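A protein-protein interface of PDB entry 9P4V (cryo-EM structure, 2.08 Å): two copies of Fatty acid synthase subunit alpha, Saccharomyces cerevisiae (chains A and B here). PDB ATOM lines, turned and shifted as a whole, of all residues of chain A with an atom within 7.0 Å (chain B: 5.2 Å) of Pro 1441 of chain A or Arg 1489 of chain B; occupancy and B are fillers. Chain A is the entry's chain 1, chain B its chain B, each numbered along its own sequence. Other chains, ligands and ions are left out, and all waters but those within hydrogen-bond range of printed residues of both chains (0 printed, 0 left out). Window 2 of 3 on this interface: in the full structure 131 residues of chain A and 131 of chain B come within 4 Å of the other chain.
The backbone NH (N) of Leu 1443 of chain A lies within hydrogen-bond range of the side-chain hydroxyl (OG) of Ser 1440 of chain A (3.4 Å). The guanidinium group (NH1) of Arg 1489 of chain B is in salt-bridge range of the side-chain carboxylate (OE1) of Glu 1473 of chain B (2.6 Å).
The side-chain carboxylate (OE1) of Glu 1492 of chain B is in salt-bridge range of the guanidinium group (NH1) of Arg 1518 of chain A.
Among the printed residues, merely in contact across the chains: Pro 1441 of chain A with Arg 1489 of chain B, Ser 1440 of chain A with Glu 1492 of chain B and Tyr 1438 of chain A with Glu 1488 of chain B.
Printed residues of chain B that touch a printed residue of chain A: Glu 1488, Arg 1489 and Glu 1492. Of the 13 printed residues of chain A, 4 touch a printed residue of chain B. Printed residues of chain A that touch a printed residue of chain B: Tyr 1438, Ser 1440, Pro 1441 and Arg 1518. Hydrophobic or aromatic side chains of chain A within 4 Å of the printed part of chain B: Pro 1441. Among the printed residues, 4 pairs touch across the chains.
No position is printed for both chains. Of the 4 pairs that touch across the chains among the printed residues, none has its exchanged pair printed and touching as well.
Pro 1441 of chain A touches one residue of chain B. Arg 1489 of chain B touches one residue of chain A. Of the printed residues of chain B, Arg 1518 of chain A touches Glu 1492 (2.7 Å). Of the printed residues of chain A, Glu 1488 of chain B touches Tyr 1438 (3.97 Å). Phe 1485 of chain B touches none of the printed residues of chain A. The nearest residue of chain A that does not touch Arg 1489 of chain B is Ala 1439 of chain A (4.5 Å).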
ATOM      1  N   TYR A1438      19.236 -21.004  19.523  1.00  0.00           N
ATOM      2  CA  TYR A1438      20.011 -20.599  20.685  1.00  0.00           C
ATOM      3  C   TYR A1438      19.699 -21.514  21.862  1.00  0.00           C
ATOM      4  O   TYR A1438      18.577 -22.010  22.006  1.00  0.00           O
ATOM      5  CB  TYR A1438      19.721 -19.142  21.060  1.00  0.00           C
ATOM      6  N   ALA A1439      20.706 -21.737  22.699  1.00  0.00           N
ATOM      7  CA  ALA A1439      20.583 -22.657  23.820  1.00  0.00           C
ATOM      8  C   ALA A1439      19.752 -22.054  24.946  1.00  0.00           C
ATOM      9  O   ALA A1439      19.783 -20.846  25.196  1.00  0.00           O
ATOM     10  CB  ALA A1439      21.963 -23.037  24.353  1.00  0.00           C
ATOM     11  N   SER A1440      19.015 -22.917  25.632  1.00  0.00           N
ATOM     12  CA  SER A1440      18.260 -22.500  26.804  1.00  0.00           C
ATOM     13  C   SER A1440      19.185 -22.438  28.015  1.00  0.00           C
ATOM     14  O   SER A1440      19.866 -23.422  28.314  1.00  0.00           O
ATOM     15  CB  SER A1440      17.114 -23.471  27.078  1.00  0.00           C
ATOM     16  OG  SER A1440      17.568 -24.626  27.760  1.00  0.00           O
ATOM     17  N   PRO A1441      19.250 -21.310  28.725  1.00  0.00           N
ATOM     18  CA  PRO A1441      20.025 -21.290  29.976  1.00  0.00           C
ATOM     19  C   PRO A1441      19.510 -22.277  31.001  1.00  0.00           C
ATOM     20  O   PRO A1441      20.269 -22.691  31.884  1.00  0.00           O
ATOM     21  CB  PRO A1441      19.877 -19.843  30.466  1.00  0.00           C
ATOM     22  CG  PRO A1441      19.453 -19.065  29.280  1.00  0.00           C
ATOM     23  CD  PRO A1441      18.663 -19.995  28.423  1.00  0.00           C
ATOM     24  N   ASN A1442      18.239 -22.665  30.912  1.00  0.00           N
ATOM     25  CA  ASN A1442      17.681 -23.617  31.865  1.00  0.00           C
ATOM     26  C   ASN A1442      18.476 -24.913  31.892  1.00  0.00           C
ATOM     27  O   ASN A1442      18.560 -25.568  32.936  1.00  0.00           O
ATOM     28  CB  ASN A1442      16.222 -23.896  31.513  1.00  0.00           C
ATOM     29  CG  ASN A1442      15.361 -24.119  32.735  1.00  0.00           C
ATOM     30  OD1 ASN A1442      15.571 -23.502  33.779  1.00  0.00           O
ATOM     31  ND2 ASN A1442      14.387 -25.007  32.611  1.00  0.00           N
ATOM     32  N   LEU A1443      19.065 -25.300  30.764  1.00  0.00           N
ATOM     33  CA  LEU A1443      19.856 -26.520  30.698  1.00  0.00           C
ATOM     34  C   LEU A1443      21.246 -26.357  31.296  1.00  0.00           C
ATOM     35  O   LEU A1443      21.923 -27.362  31.521  1.00  0.00           O
ATOM     36  CB  LEU A1443      19.968 -26.978  29.243  1.00  0.00           C
ATOM     37  CG  LEU A1443      20.023 -28.475  28.940  1.00  0.00           C
ATOM     38  CD1 LEU A1443      18.873 -29.240  29.574  1.00  0.00           C
ATOM     39  CD2 LEU A1443      20.018 -28.676  27.435  1.00  0.00           C
ATOM     40  N   ASN A1444      21.681 -25.132  31.572  1.00  0.00           N
ATOM     41  CA  ASN A1444      23.013 -24.881  32.108  1.00  0.00           C
ATOM     42  C   ASN A1444      22.959 -24.841  33.630  1.00  0.00           C
ATOM     43  O   ASN A1444      22.238 -24.023  34.207  1.00  0.00           O
ATOM     44  CB  ASN A1444      23.566 -23.569  31.563  1.00  0.00           C
ATOM     45  CG  ASN A1444      24.946 -23.266  32.088  1.00  0.00           C
ATOM     46  OD1 ASN A1444      25.176 -22.228  32.700  1.00  0.00           O
ATOM     47  ND2 ASN A1444      25.877 -24.180  31.857  1.00  0.00           N
ATOM     48  N   MET A1445      23.744 -25.704  34.277  1.00  0.00           N
ATOM     49  CA  MET A1445      23.665 -25.815  35.729  1.00  0.00           C
ATOM     50  C   MET A1445      24.280 -24.609  36.426  1.00  0.00           C
ATOM     51  O   MET A1445      23.852 -24.251  37.524  1.00  0.00           O
ATOM     52  CB  MET A1445      24.346 -27.104  36.196  1.00  0.00           C
ATOM     53  CG  MET A1445      24.570 -27.161  37.701  1.00  0.00           C
ATOM     54  SD  MET A1445      24.999 -28.767  38.416  1.00  0.00           S
ATOM     55  CE  MET A1445      24.214 -29.936  37.322  1.00  0.00           C
ATOM     56  N   LYS A1446      25.282 -23.974  35.822  1.00  0.00           N
ATOM     57  CA  LYS A1446      25.850 -22.779  36.433  1.00  0.00           C
ATOM     58  C   LYS A1446      24.819 -21.670  36.535  1.00  0.00           C
ATOM     59  O   LYS A1446      24.857 -20.865  37.469  1.00  0.00           O
ATOM     60  CB  LYS A1446      27.053 -22.294  35.629  1.00  0.00           C
ATOM     61  CG  LYS A1446      28.390 -22.697  36.227  1.00  0.00           C
ATOM     62  CD  LYS A1446      29.592 -22.006  35.574  1.00  0.00           C
ATOM     63  CE  LYS A1446      29.524 -20.478  35.604  1.00  0.00           C
ATOM     64  NZ  LYS A1446      30.411 -19.900  36.652  1.00  0.00           N
ATOM     65  N   TYR A1447      23.897 -21.609  35.576  1.00  0.00           N
ATOM     66  CA  TYR A1447      22.866 -20.587  35.603  1.00  0.00           C
ATOM     67  C   TYR A1447      21.808 -20.896  36.656  1.00  0.00           C
ATOM     68  O   TYR A1447      21.345 -19.994  37.361  1.00  0.00           O
ATOM     69  CB  TYR A1447      22.243 -20.468  34.217  1.00  0.00           C
ATOM     70  CG  TYR A1447      20.907 -19.792  34.209  1.00  0.00           C
ATOM     71  CD1 TYR A1447      20.811 -18.412  34.227  1.00  0.00           C
ATOM     72  CD2 TYR A1447      19.740 -20.531  34.178  1.00  0.00           C
ATOM     73  CE1 TYR A1447      19.593 -17.793  34.217  1.00  0.00           C
ATOM     74  CE2 TYR A1447      18.516 -19.917  34.172  1.00  0.00           C
ATOM     75  CZ  TYR A1447      18.447 -18.547  34.188  1.00  0.00           C
ATOM     76  OH  TYR A1447      17.228 -17.919  34.179  1.00  0.00           O
ATOM     77  N   ARG A1448      21.439 -22.163  36.790  1.00  0.00           N
ATOM     78  CA  ARG A1448      20.465 -22.542  37.795  1.00  0.00           C
ATOM     79  C   ARG A1448      21.018 -22.308  39.206  1.00  0.00           C
ATOM     80  O   ARG A1448      20.282 -21.885  40.091  1.00  0.00           O
ATOM     81  CB  ARG A1448      20.047 -23.999  37.607  1.00  0.00           C
ATOM     82  CG  ARG A1448      19.418 -24.292  36.256  1.00  0.00           C
ATOM     83  CD  ARG A1448      18.667 -25.611  36.262  1.00  0.00           C
ATOM     84  NE  ARG A1448      19.514 -26.733  36.664  1.00  0.00           N
ATOM     85  CZ  ARG A1448      20.293 -27.431  35.844  1.00  0.00           C
ATOM     86  NH1 ARG A1448      20.360 -27.137  34.554  1.00  0.00           N
ATOM     87  NH2 ARG A1448      21.016 -28.433  36.321  1.00  0.00           N
ATOM     88  N   PHE A1512      13.740 -28.302  37.312  1.00  0.00           N
ATOM     89  CA  PHE A1512      13.906 -27.127  36.457  1.00  0.00           C
ATOM     90  C   PHE A1512      13.364 -27.300  35.056  1.00  0.00           C
ATOM     91  O   PHE A1512      13.044 -26.327  34.428  1.00  0.00           O
ATOM     92  CB  PHE A1512      15.392 -26.781  36.388  1.00  0.00           C
ATOM     93  CG  PHE A1512      16.231 -27.839  35.733  1.00  0.00           C
ATOM     94  CD1 PHE A1512      16.785 -28.864  36.480  1.00  0.00           C
ATOM     95  CD2 PHE A1512      16.466 -27.805  34.371  1.00  0.00           C
ATOM     96  CE1 PHE A1512      17.556 -29.839  35.878  1.00  0.00           C
ATOM     97  CE2 PHE A1512      17.237 -28.775  33.763  1.00  0.00           C
ATOM     98  CZ  PHE A1512      17.783 -29.794  34.517  1.00  0.00           C
ATOM     99  N   ARG A1518      11.072 -27.827  25.662  1.00  0.00           N
ATOM    100  CA  ARG A1518      12.295 -28.062  24.916  1.00  0.00           C
ATOM    101  C   ARG A1518      13.259 -28.996  25.636  1.00  0.00           C
ATOM    102  O   ARG A1518      14.387 -29.170  25.171  1.00  0.00           O
ATOM    103  CB  ARG A1518      12.997 -26.738  24.621  1.00  0.00           C
ATOM    104  CG  ARG A1518      12.050 -25.594  24.352  1.00  0.00           C
ATOM    105  CD  ARG A1518      12.619 -24.614  23.354  1.00  0.00           C
ATOM    106  NE  ARG A1518      13.795 -23.917  23.858  1.00  0.00           N
ATOM    107  CZ  ARG A1518      13.784 -23.039  24.853  1.00  0.00           C
ATOM    108  NH1 ARG A1518      12.674 -22.745  25.510  1.00  0.00           N
ATOM    109  NH2 ARG A1518      14.916 -22.433  25.194  1.00  0.00           N
ATOM    110  N   LEU B1470      18.379  -9.671  29.410  1.00  0.00           N
ATOM    111  CA  LEU B1470      18.201 -10.192  28.062  1.00  0.00           C
ATOM    112  C   LEU B1470      18.319  -9.076  27.029  1.00  0.00           C
ATOM    113  O   LEU B1470      18.944  -9.256  25.977  1.00  0.00           O
ATOM    114  CB  LEU B1470      16.845 -10.886  27.952  1.00  0.00           C
ATOM    115  CG  LEU B1470      16.474 -11.506  26.604  1.00  0.00           C
ATOM    116  CD1 LEU B1470      17.515 -12.530  26.193  1.00  0.00           C
ATOM    117  CD2 LEU B1470      15.091 -12.142  26.668  1.00  0.00           C
ATOM    118  N   GLU B1473      21.789  -8.757  26.291  1.00  0.00           N
ATOM    119  CA  GLU B1473      22.263  -9.915  25.542  1.00  0.00           C
ATOM    120  C   GLU B1473      21.896  -9.822  24.068  1.00  0.00           C
ATOM    121  O   GLU B1473      22.507 -10.509  23.241  1.00  0.00           O
ATOM    122  CB  GLU B1473      21.682 -11.208  26.122  1.00  0.00           C
ATOM    123  CG  GLU B1473      22.226 -11.611  27.481  1.00  0.00           C
ATOM    124  CD  GLU B1473      21.757 -12.998  27.898  1.00  0.00           C
ATOM    125  OE1 GLU B1473      21.637 -13.876  27.018  1.00  0.00           O
ATOM    126  OE2 GLU B1473      21.494 -13.210  29.102  1.00  0.00           O
ATOM    127  N   GLU B1484      14.385 -13.412  16.475  1.00  0.00           N
ATOM    128  CA  GLU B1484      14.392 -14.812  16.884  1.00  0.00           C
ATOM    129  C   GLU B1484      15.011 -14.976  18.266  1.00  0.00           C
ATOM    130  O   GLU B1484      14.489 -15.716  19.106  1.00  0.00           O
ATOM    131  CB  GLU B1484      15.145 -15.654  15.855  1.00  0.00           C
ATOM    132  N   PHE B1485      16.117 -14.280  18.525  1.00  0.00           N
ATOM    133  CA  PHE B1485      16.775 -14.390  19.822  1.00  0.00           C
ATOM    134  C   PHE B1485      15.856 -13.935  20.948  1.00  0.00           C
ATOM    135  O   PHE B1485      15.789 -14.578  22.002  1.00  0.00           O
ATOM    136  CB  PHE B1485      18.063 -13.572  19.809  1.00  0.00           C
ATOM    137  CG  PHE B1485      18.645 -13.317  21.168  1.00  0.00           C
ATOM    138  CD1 PHE B1485      19.441 -14.264  21.786  1.00  0.00           C
ATOM    139  CD2 PHE B1485      18.422 -12.113  21.813  1.00  0.00           C
ATOM    140  CE1 PHE B1485      19.990 -14.022  23.026  1.00  0.00           C
ATOM    141  CE2 PHE B1485      18.970 -11.867  23.054  1.00  0.00           C
ATOM    142  CZ  PHE B1485      19.756 -12.823  23.661  1.00  0.00           C
ATOM    143  N   LEU B1486      15.133 -12.832  20.743  1.00  0.00           N
ATOM    144  CA  LEU B1486      14.317 -12.270  21.815  1.00  0.00           C
ATOM    145  C   LEU B1486      13.100 -13.143  22.106  1.00  0.00           C
ATOM    146  O   LEU B1486      12.773 -13.397  23.269  1.00  0.00           O
ATOM    147  CB  LEU B1486      13.885 -10.852  21.449  1.00  0.00           C
ATOM    148  CG  LEU B1486      14.146  -9.751  22.479  1.00  0.00           C
ATOM    149  CD1 LEU B1486      15.606  -9.713  22.919  1.00  0.00           C
ATOM    150  CD2 LEU B1486      13.731  -8.413  21.900  1.00  0.00           C
ATOM    151  N   LEU B1487      12.408 -13.601  21.061  1.00  0.00           N
ATOM    152  CA  LEU B1487      11.212 -14.411  21.271  1.00  0.00           C
ATOM    153  C   LEU B1487      11.537 -15.708  22.002  1.00  0.00           C
ATOM    154  O   LEU B1487      10.778 -16.138  22.876  1.00  0.00           O
ATOM    155  CB  LEU B1487      10.530 -14.717  19.937  1.00  0.00           C
ATOM    156  CG  LEU B1487       9.902 -13.537  19.198  1.00  0.00           C
ATOM    157  CD1 LEU B1487       9.709 -13.883  17.732  1.00  0.00           C
ATOM    158  CD2 LEU B1487       8.575 -13.149  19.840  1.00  0.00           C
ATOM    159  N   GLU B1488      12.651 -16.355  21.654  1.00  0.00           N
ATOM    160  CA  GLU B1488      12.975 -17.623  22.300  1.00  0.00           C
ATOM    161  C   GLU B1488      13.367 -17.415  23.758  1.00  0.00           C
ATOM    162  O   GLU B1488      12.934 -18.170  24.635  1.00  0.00           O
ATOM    163  CB  GLU B1488      14.089 -18.344  21.540  1.00  0.00           C
ATOM    164  CG  GLU B1488      13.691 -18.781  20.137  1.00  0.00           C
ATOM    165  CD  GLU B1488      14.432 -20.020  19.658  1.00  0.00           C
ATOM    166  OE1 GLU B1488      15.204 -20.608  20.446  1.00  0.00           O
ATOM    167  OE2 GLU B1488      14.238 -20.408  18.488  1.00  0.00           O
ATOM    168  N   ARG B1489      14.179 -16.394  24.038  1.00  0.00           N
ATOM    169  CA  ARG B1489      14.586 -16.137  25.416  1.00  0.00           C
ATOM    170  C   ARG B1489      13.436 -15.572  26.239  1.00  0.00           C
ATOM    171  O   ARG B1489      13.287 -15.914  27.418  1.00  0.00           O
ATOM    172  CB  ARG B1489      15.781 -15.185  25.439  1.00  0.00           C
ATOM    173  CG  ARG B1489      17.032 -15.751  24.778  1.00  0.00           C
ATOM    174  CD  ARG B1489      17.604 -16.964  25.511  1.00  0.00           C
ATOM    175  NE  ARG B1489      17.676 -16.774  26.955  1.00  0.00           N
ATOM    176  CZ  ARG B1489      18.511 -15.940  27.562  1.00  0.00           C
ATOM    177  NH1 ARG B1489      19.348 -15.177  26.880  1.00  0.00           N
ATOM    178  NH2 ARG B1489      18.510 -15.874  28.890  1.00  0.00           N
ATOM    179  N   THR B1490      12.611 -14.710  25.642  1.00  0.00           N
ATOM    180  CA  THR B1490      11.505 -14.116  26.389  1.00  0.00           C
ATOM    181  C   THR B1490      10.511 -15.176  26.848  1.00  0.00           C
ATOM    182  O   THR B1490      10.026 -15.131  27.983  1.00  0.00           O
ATOM    183  CB  THR B1490      10.802 -13.057  25.541  1.00  0.00           C
ATOM    184  OG1 THR B1490      11.703 -11.975  25.289  1.00  0.00           O
ATOM    185  CG2 THR B1490       9.569 -12.526  26.258  1.00  0.00           C
ATOM    186  N   ARG B1491      10.190 -16.138  25.981  1.00  0.00           N
ATOM    187  CA  ARG B1491       9.273 -17.203  26.378  1.00  0.00           C
ATOM    188  C   ARG B1491       9.776 -17.926  27.622  1.00  0.00           C
ATOM    189  O   ARG B1491       8.979 -18.335  28.474  1.00  0.00           O
ATOM    190  CB  ARG B1491       9.091 -18.196  25.230  1.00  0.00           C
ATOM    191  CG  ARG B1491       7.709 -18.833  25.142  1.00  0.00           C
ATOM    192  CD  ARG B1491       7.736 -20.310  25.529  1.00  0.00           C
ATOM    193  NE  ARG B1491       6.495 -20.999  25.184  1.00  0.00           N
ATOM    194  CZ  ARG B1491       6.187 -22.233  25.562  1.00  0.00           C
ATOM    195  NH1 ARG B1491       7.005 -22.954  26.310  1.00  0.00           N
ATOM    196  NH2 ARG B1491       5.030 -22.763  25.170  1.00  0.00           N
ATOM    197  N   GLU B1492      11.094 -18.102  27.738  1.00  0.00           N
ATOM    198  CA  GLU B1492      11.651 -18.863  28.852  1.00  0.00           C
ATOM    199  C   GLU B1492      11.583 -18.077  30.159  1.00  0.00           C
ATOM    200  O   GLU B1492      11.218 -18.626  31.204  1.00  0.00           O
ATOM    201  CB  GLU B1492      13.092 -19.268  28.533  1.00  0.00           C
ATOM    202  CG  GLU B1492      13.681 -20.299  29.485  1.00  0.00           C
ATOM    203  CD  GLU B1492      13.258 -21.724  29.162  1.00  0.00           C
ATOM    204  OE1 GLU B1492      13.545 -22.200  28.038  1.00  0.00           O
ATOM    205  OE2 GLU B1492      12.638 -22.370  30.036  1.00  0.00           O
ATOM    206  N   ILE B1493      11.938 -16.791  30.127  1.00  0.00           N
ATOM    207  CA  ILE B1493      11.927 -15.997  31.353  1.00  0.00           C
ATOM    208  C   ILE B1493      10.520 -15.920  31.932  1.00  0.00           C
ATOM    209  O   ILE B1493      10.325 -16.050  33.146  1.00  0.00           O
ATOM    210  CB  ILE B1493      12.504 -14.591  31.103  1.00  0.00           C
ATOM    211  CG1 ILE B1493      12.313 -13.718  32.345  1.00  0.00           C
ATOM    212  CG2 ILE B1493      11.850 -13.941  29.890  1.00  0.00           C
ATOM    213  CD1 ILE B1493      12.811 -12.315  32.187  1.00  0.00           C
